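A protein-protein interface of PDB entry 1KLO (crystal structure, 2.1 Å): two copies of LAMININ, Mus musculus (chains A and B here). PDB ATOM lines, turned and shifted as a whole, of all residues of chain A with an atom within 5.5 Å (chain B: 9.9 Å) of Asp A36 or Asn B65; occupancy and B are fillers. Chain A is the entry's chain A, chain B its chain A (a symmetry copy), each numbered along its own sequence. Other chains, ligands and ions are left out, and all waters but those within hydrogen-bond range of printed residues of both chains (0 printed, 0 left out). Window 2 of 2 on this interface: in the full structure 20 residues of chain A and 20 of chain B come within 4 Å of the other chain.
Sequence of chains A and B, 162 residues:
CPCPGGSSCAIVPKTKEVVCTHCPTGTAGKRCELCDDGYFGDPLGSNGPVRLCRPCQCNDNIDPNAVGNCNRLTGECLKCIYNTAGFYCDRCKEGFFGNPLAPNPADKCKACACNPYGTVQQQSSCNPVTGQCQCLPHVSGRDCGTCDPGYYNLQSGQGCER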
ATOM      1  N   GLY A  26     -30.522   1.775 -13.466  1.00  0.00           N
ATOM      2  CA  GLY A  26     -29.111   1.588 -13.195  1.00  0.00           C
ATOM      3  C   GLY A  26     -28.540   2.759 -12.419  1.00  0.00           C
ATOM      4  O   GLY A  26     -27.524   2.630 -11.748  1.00  0.00           O
ATOM      5  N   THR A  27     -29.202   3.907 -12.499  1.00  0.00           N
ATOM      6  CA  THR A  27     -28.742   5.114 -11.814  1.00  0.00           C
ATOM      7  C   THR A  27     -29.694   5.543 -10.713  1.00  0.00           C
ATOM      8  O   THR A  27     -30.869   5.175 -10.706  1.00  0.00           O
ATOM      9  CB  THR A  27     -28.626   6.269 -12.779  1.00  0.00           C
ATOM     10  OG1 THR A  27     -29.942   6.679 -13.174  1.00  0.00           O
ATOM     11  CG2 THR A  27     -27.854   5.838 -14.008  1.00  0.00           C
ATOM     12  N   ALA A  28     -29.184   6.362  -9.813  1.00  0.00           N
ATOM     13  CA  ALA A  28     -29.952   6.832  -8.696  1.00  0.00           C
ATOM     14  C   ALA A  28     -29.357   8.163  -8.290  1.00  0.00           C
ATOM     15  O   ALA A  28     -28.487   8.684  -8.976  1.00  0.00           O
ATOM     16  CB  ALA A  28     -29.840   5.842  -7.565  1.00  0.00           C
ATOM     17  N   LEU A  34     -25.543   8.913  -9.375  1.00  0.00           N
ATOM     18  CA  LEU A  34     -24.978   7.721  -8.737  1.00  0.00           C
ATOM     19  C   LEU A  34     -25.499   6.498  -9.453  1.00  0.00           C
ATOM     20  O   LEU A  34     -26.507   6.578 -10.161  1.00  0.00           O
ATOM     21  CB  LEU A  34     -25.452   7.586  -7.307  1.00  0.00           C
ATOM     22  CG  LEU A  34     -25.161   8.714  -6.350  1.00  0.00           C
ATOM     23  CD1 LEU A  34     -25.816   8.395  -5.018  1.00  0.00           C
ATOM     24  CD2 LEU A  34     -23.665   8.872  -6.200  1.00  0.00           C
ATOM     25  N   CYS A  35     -24.814   5.368  -9.296  1.00  0.00           N
ATOM     26  CA  CYS A  35     -25.327   4.140  -9.888  1.00  0.00           C
ATOM     27  C   CYS A  35     -26.155   3.518  -8.791  1.00  0.00           C
ATOM     28  O   CYS A  35     -25.881   3.685  -7.609  1.00  0.00           O
ATOM     29  CB  CYS A  35     -24.222   3.191 -10.309  1.00  0.00           C
ATOM     30  SG  CYS A  35     -23.327   3.706 -11.800  1.00  0.00           S
ATOM     31  N   ASP A  36     -27.206   2.846  -9.199  1.00  0.00           N
ATOM     32  CA  ASP A  36     -28.128   2.192  -8.291  1.00  0.00           C
ATOM     33  C   ASP A  36     -27.438   1.005  -7.624  1.00  0.00           C
ATOM     34  O   ASP A  36     -26.434   0.502  -8.136  1.00  0.00           O
ATOM     35  CB  ASP A  36     -29.327   1.702  -9.117  1.00  0.00           C
ATOM     36  CG  ASP A  36     -30.590   1.475  -8.283  1.00  0.00           C
ATOM     37  OD1 ASP A  36     -30.571   1.662  -7.032  1.00  0.00           O
ATOM     38  OD2 ASP A  36     -31.611   1.110  -8.924  1.00  0.00           O
ATOM     39  N   ASP A  37     -27.977   0.541  -6.502  1.00  0.00           N
ATOM     40  CA  ASP A  37     -27.401  -0.605  -5.811  1.00  0.00           C
ATOM     41  C   ASP A  37     -27.369  -1.795  -6.751  1.00  0.00           C
ATOM     42  O   ASP A  37     -28.307  -2.041  -7.515  1.00  0.00           O
ATOM     43  CB  ASP A  37     -28.230  -0.970  -4.593  1.00  0.00           C
ATOM     44  CG  ASP A  37     -27.590  -2.053  -3.747  1.00  0.00           C
ATOM     45  OD1 ASP A  37     -26.522  -1.779  -3.141  1.00  0.00           O
ATOM     46  OD2 ASP A  37     -28.177  -3.162  -3.685  1.00  0.00           O
ATOM     47  N   GLY A  38     -26.273  -2.529  -6.687  1.00  0.00           N
ATOM     48  CA  GLY A  38     -26.124  -3.676  -7.544  1.00  0.00           C
ATOM     49  C   GLY A  38     -25.439  -3.295  -8.826  1.00  0.00           C
ATOM     50  O   GLY A  38     -25.185  -4.164  -9.663  1.00  0.00           O
ATOM     51  N   TYR A  39     -25.129  -2.005  -8.972  1.00  0.00           N
ATOM     52  CA  TYR A  39     -24.482  -1.484 -10.169  1.00  0.00           C
ATOM     53  C   TYR A  39     -23.260  -0.691  -9.794  1.00  0.00           C
ATOM     54  O   TYR A  39     -23.089  -0.365  -8.632  1.00  0.00           O
ATOM     55  CB  TYR A  39     -25.422  -0.536 -10.914  1.00  0.00           C
ATOM     56  CG  TYR A  39     -26.568  -1.192 -11.610  1.00  0.00           C
ATOM     57  CD1 TYR A  39     -27.672  -1.669 -10.902  1.00  0.00           C
ATOM     58  CD2 TYR A  39     -26.570  -1.321 -12.982  1.00  0.00           C
ATOM     59  CE1 TYR A  39     -28.754  -2.262 -11.560  1.00  0.00           C
ATOM     60  CE2 TYR A  39     -27.647  -1.911 -13.651  1.00  0.00           C
ATOM     61  CZ  TYR A  39     -28.731  -2.374 -12.929  1.00  0.00           C
ATOM     62  OH  TYR A  39     -29.781  -2.940 -13.613  1.00  0.00           O
ATOM     63  N   PHE A  40     -22.396  -0.415 -10.772  1.00  0.00           N
ATOM     64  CA  PHE A  40     -21.233   0.432 -10.530  1.00  0.00           C
ATOM     65  C   PHE A  40     -20.889   1.210 -11.798  1.00  0.00           C
ATOM     66  O   PHE A  40     -21.293   0.830 -12.912  1.00  0.00           O
ATOM     67  CB  PHE A  40     -20.043  -0.349  -9.968  1.00  0.00           C
ATOM     68  CG  PHE A  40     -19.296  -1.135 -10.982  1.00  0.00           C
ATOM     69  CD1 PHE A  40     -19.764  -2.367 -11.404  1.00  0.00           C
ATOM     70  CD2 PHE A  40     -18.109  -0.647 -11.517  1.00  0.00           C
ATOM     71  CE1 PHE A  40     -19.067  -3.109 -12.347  1.00  0.00           C
ATOM     72  CE2 PHE A  40     -17.397  -1.391 -12.471  1.00  0.00           C
ATOM     73  CZ  PHE A  40     -17.885  -2.626 -12.882  1.00  0.00           C
ATOM     74  N   CYS A  53     -23.421   2.810 -15.897  1.00  0.00           N
ATOM     75  CA  CYS A  53     -23.637   1.924 -14.780  1.00  0.00           C
ATOM     76  C   CYS A  53     -23.877   0.550 -15.352  1.00  0.00           C
ATOM     77  O   CYS A  53     -24.586   0.404 -16.349  1.00  0.00           O
ATOM     78  CB  CYS A  53     -24.858   2.361 -13.986  1.00  0.00           C
ATOM     79  SG  CYS A  53     -24.682   3.989 -13.234  1.00  0.00           S
ATOM     80  N   ARG A  72     -20.272   1.024  -5.491  1.00  0.00           N
ATOM     81  CA  ARG A  72     -20.954   1.710  -6.580  1.00  0.00           C
ATOM     82  C   ARG A  72     -20.052   2.510  -7.502  1.00  0.00           C
ATOM     83  O   ARG A  72     -20.454   2.852  -8.596  1.00  0.00           O
ATOM     84  CB  ARG A  72     -22.045   2.613  -6.021  1.00  0.00           C
ATOM     85  CG  ARG A  72     -23.290   1.886  -5.435  1.00  0.00           C
ATOM     86  CD  ARG A  72     -24.074   2.873  -4.522  1.00  0.00           C
ATOM     87  NE  ARG A  72     -25.510   2.622  -4.371  1.00  0.00           N
ATOM     88  CZ  ARG A  72     -26.456   3.494  -4.732  1.00  0.00           C
ATOM     89  NH1 ARG A  72     -26.123   4.649  -5.291  1.00  0.00           N
ATOM     90  NH2 ARG A  72     -27.741   3.209  -4.554  1.00  0.00           N
ATOM     91  N   ASP B  37     -35.966 -17.080  -6.277  1.00  0.00           N
ATOM     92  CA  ASP B  37     -35.761 -16.295  -7.486  1.00  0.00           C
ATOM     93  C   ASP B  37     -34.335 -15.777  -7.516  1.00  0.00           C
ATOM     94  O   ASP B  37     -33.780 -15.355  -6.498  1.00  0.00           O
ATOM     95  CB  ASP B  37     -36.709 -15.110  -7.524  1.00  0.00           C
ATOM     96  CG  ASP B  37     -36.650 -14.348  -8.834  1.00  0.00           C
ATOM     97  OD1 ASP B  37     -37.067 -14.924  -9.873  1.00  0.00           O
ATOM     98  OD2 ASP B  37     -36.203 -13.175  -8.803  1.00  0.00           O
ATOM     99  N   GLY B  38     -33.749 -15.820  -8.698  1.00  0.00           N
ATOM    100  CA  GLY B  38     -32.389 -15.371  -8.844  1.00  0.00           C
ATOM    101  C   GLY B  38     -31.429 -16.511  -8.655  1.00  0.00           C
ATOM    102  O   GLY B  38     -30.219 -16.319  -8.791  1.00  0.00           O
ATOM    103  N   ASN B  61     -25.149 -10.017 -17.389  1.00  0.00           N
ATOM    104  CA  ASN B  61     -25.935  -9.287 -18.347  1.00  0.00           C
ATOM    105  C   ASN B  61     -27.422  -9.358 -18.016  1.00  0.00           C
ATOM    106  O   ASN B  61     -28.251  -9.455 -18.911  1.00  0.00           O
ATOM    107  CB  ASN B  61     -25.678  -9.833 -19.759  1.00  0.00           C
ATOM    108  CG  ASN B  61     -24.299  -9.461 -20.295  1.00  0.00           C
ATOM    109  OD1 ASN B  61     -23.735  -8.437 -19.936  1.00  0.00           O
ATOM    110  ND2 ASN B  61     -23.758 -10.297 -21.162  1.00  0.00           N
ATOM    111  N   ILE B  62     -27.747  -9.336 -16.722  1.00  0.00           N
ATOM    112  CA  ILE B  62     -29.138  -9.351 -16.232  1.00  0.00           C
ATOM    113  C   ILE B  62     -29.278  -8.274 -15.151  1.00  0.00           C
ATOM    114  O   ILE B  62     -28.327  -7.989 -14.420  1.00  0.00           O
ATOM    115  CB  ILE B  62     -29.586 -10.729 -15.605  1.00  0.00           C
ATOM    116  CG1 ILE B  62     -28.573 -11.209 -14.568  1.00  0.00           C
ATOM    117  CG2 ILE B  62     -29.881 -11.721 -16.693  1.00  0.00           C
ATOM    118  CD1 ILE B  62     -29.026 -12.382 -13.774  1.00  0.00           C
ATOM    119  N   ASP B  63     -30.465  -7.688 -15.057  1.00  0.00           N
ATOM    120  CA  ASP B  63     -30.759  -6.637 -14.091  1.00  0.00           C
ATOM    121  C   ASP B  63     -30.834  -7.283 -12.732  1.00  0.00           C
ATOM    122  O   ASP B  63     -31.696  -8.122 -12.482  1.00  0.00           O
ATOM    123  CB  ASP B  63     -32.095  -5.985 -14.446  1.00  0.00           C
ATOM    124  CG  ASP B  63     -32.455  -4.808 -13.545  1.00  0.00           C
ATOM    125  OD1 ASP B  63     -31.712  -4.482 -12.590  1.00  0.00           O
ATOM    126  OD2 ASP B  63     -33.520  -4.200 -13.806  1.00  0.00           O
ATOM    127  N   PRO B  64     -29.957  -6.868 -11.817  1.00  0.00           N
ATOM    128  CA  PRO B  64     -29.890  -7.402 -10.451  1.00  0.00           C
ATOM    129  C   PRO B  64     -31.183  -7.196  -9.694  1.00  0.00           C
ATOM    130  O   PRO B  64     -31.455  -7.880  -8.715  1.00  0.00           O
ATOM    131  CB  PRO B  64     -28.786  -6.582  -9.803  1.00  0.00           C
ATOM    132  CG  PRO B  64     -28.013  -6.037 -10.946  1.00  0.00           C
ATOM    133  CD  PRO B  64     -29.019  -5.753 -11.992  1.00  0.00           C
ATOM    134  N   ASN B  65     -31.966  -6.231 -10.138  1.00  0.00           N
ATOM    135  CA  ASN B  65     -33.208  -5.901  -9.468  1.00  0.00           C
ATOM    136  C   ASN B  65     -34.455  -6.371 -10.216  1.00  0.00           C
ATOM    137  O   ASN B  65     -35.556  -5.913  -9.932  1.00  0.00           O
ATOM    138  CB  ASN B  65     -33.273  -4.379  -9.220  1.00  0.00           C
ATOM    139  CG  ASN B  65     -32.066  -3.839  -8.413  1.00  0.00           C
ATOM    140  OD1 ASN B  65     -31.558  -2.745  -8.705  1.00  0.00           O
ATOM    141  ND2 ASN B  65     -31.612  -4.601  -7.401  1.00  0.00           N
ATOM    142  N   ALA B  66     -34.290  -7.259 -11.184  1.00  0.00           N
ATOM    143  CA  ALA B  66     -35.436  -7.772 -11.913  1.00  0.00           C
ATOM    144  C   ALA B  66     -35.782  -9.121 -11.289  1.00  0.00           C
ATOM    145  O   ALA B  66     -35.017  -9.659 -10.469  1.00  0.00           O
ATOM    146  CB  ALA B  66     -35.100  -7.948 -13.379  1.00  0.00           C
ATOM    147  N   VAL B  67     -36.933  -9.665 -11.659  1.00  0.00           N
ATOM    148  CA  VAL B  67     -37.345 -10.960 -11.143  1.00  0.00           C
ATOM    149  C   VAL B  67     -37.495 -11.883 -12.326  1.00  0.00           C
ATOM    150  O   VAL B  67     -37.794 -11.430 -13.420  1.00  0.00           O
ATOM    151  CB  VAL B  67     -38.696 -10.896 -10.341  1.00  0.00           C
ATOM    152  CG1 VAL B  67     -38.556  -9.966  -9.162  1.00  0.00           C
ATOM    153  CG2 VAL B  67     -39.835 -10.448 -11.232  1.00  0.00           C
ATOM    154  N   GLY B  68     -37.238 -13.168 -12.115  1.00  0.00           N
ATOM    155  CA  GLY B  68     -37.373 -14.130 -13.189  1.00  0.00           C
ATOM    156  C   GLY B  68     -36.252 -14.050 -14.195  1.00  0.00           C
ATOM    157  O   GLY B  68     -36.442 -14.341 -15.370  1.00  0.00           O
ATOM    158  N   ASN B  69     -35.065 -13.685 -13.730  1.00  0.00           N
ATOM    159  CA  ASN B  69     -33.921 -13.562 -14.613  1.00  0.00           C
ATOM    160  C   ASN B  69     -33.493 -14.882 -15.197  1.00  0.00           C
ATOM    161  O   ASN B  69     -32.967 -14.925 -16.284  1.00  0.00           O
ATOM    162  CB  ASN B  69     -32.772 -12.889 -13.885  1.00  0.00           C
ATOM    163  CG  ASN B  69     -32.935 -11.395 -13.830  1.00  0.00           C
ATOM    164  OD1 ASN B  69     -33.520 -10.791 -14.725  1.00  0.00           O
ATOM    165  ND2 ASN B  69     -32.433 -10.790 -12.780  1.00  0.00           N
ATOM    166  N   LYS B  79     -33.953 -13.059 -18.938  1.00  0.00           N
ATOM    167  CA  LYS B  79     -34.083 -11.635 -19.122  1.00  0.00           C
ATOM    168  C   LYS B  79     -32.757 -10.964 -19.379  1.00  0.00           C
ATOM    169  O   LYS B  79     -32.335 -10.122 -18.572  1.00  0.00           O
ATOM    170  CB  LYS B  79     -34.729 -11.026 -17.893  1.00  0.00           C
ATOM    171  CG  LYS B  79     -36.129 -11.464 -17.697  1.00  0.00           C
ATOM    172  CD  LYS B  79     -36.697 -10.688 -16.575  1.00  0.00           C
ATOM    173  CE  LYS B  79     -38.185 -10.853 -16.539  1.00  0.00           C
ATOM    174  NZ  LYS B  79     -38.771  -9.957 -15.504  1.00  0.00           N
ATOM    175  N   ILE B  81     -30.114  -8.409 -20.743  1.00  0.00           N
ATOM    176  CA  ILE B  81     -30.204  -6.995 -21.109  1.00  0.00           C
ATOM    177  C   ILE B  81     -29.052  -6.578 -22.004  1.00  0.00           C
ATOM    178  O   ILE B  81     -28.173  -7.383 -22.295  1.00  0.00           O
ATOM    179  CB  ILE B  81     -30.235  -6.097 -19.878  1.00  0.00           C
ATOM    180  CG1 ILE B  81     -28.961  -6.243 -19.055  1.00  0.00           C
ATOM    181  CG2 ILE B  81     -31.410  -6.473 -19.018  1.00  0.00           C
ATOM    182  CD1 ILE B  81     -28.911  -5.296 -17.853  1.00  0.00           C
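The side-chain carboxylate (OD1) of Asp B63 is in hydrogen-bond range of the side-chain hydroxyl (OH) of Tyr A39.
The side-chain amide nitrogen of Asn B69 lies within hydrogen-bond range of the backbone carbonyl oxygen of Asp B63.
The side-chain sulfur (SG) of Cys A35 forms a disulfide with the side-chain sulfur (SG) of Cys A53 (2.0 Å).
The side-chain carboxylate (OD1) of Asp B63 lies close to the backbone NH (N) of Asn B65, at 3.0 Å.
The backbone carbonyl oxygen (O) of Gly A26 is in hydrogen-bond range of the backbone NH (N) of Asp A36.
Asp A36 touches Asn B65.
Asn B65 touches Asp A37.
O of Gly A38 touches CG of Pro B64, at 3.6 Å.
CD of Pro B64 touches OH of Tyr A39, at 3.3 Å.
Of chain B, only Asn B65 (3.9 Å) comes within 4 Å of Asp A36.
Asn B65 touches just these residues of chain A: Asp A36 (3.9 Å) and Asp A37 (3.5 Å).
No residue of chain B comes within 4 Å of Cys A35.
Of chain B, only Pro B64 (3.6 Å) comes within 4 Å of Gly A38.
Of the printed residues of chain A, Asp B63 touches Tyr A39 (2.7 Å).
Of the printed residues of chain B, Tyr A39 touches Asp B63 (2.7 Å) and Pro B64 (3.3 Å).
Thr A27 touches none of the printed residues of chain B.
Arg A72 touches none of the printed residues of chain B.
The nearest residue of chain B that does not touch Asp A36 is Asp B63 (6.7 Å).
The nearest printed residue of chain A that does not touch Pro B64 is Asp A37 (5.1 Å).
Of the 13 printed residues of chain B, 3 touch a printed residue of chain A.
Hydrophobic or aromatic side chains of chain B that line the printed part of chain A: Pro B64.
Among the printed residues, 5 pairs touch across the chains.
Among the printed residues, no Asp or Glu carboxylate lies within 4 Å of a Lys or Arg side-chain nitrogen of the other chain.
2 positions are printed for both chains.
Of the 5 pairs that touch across the chains among the printed residues, none has its exchanged pair printed and touching as well.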
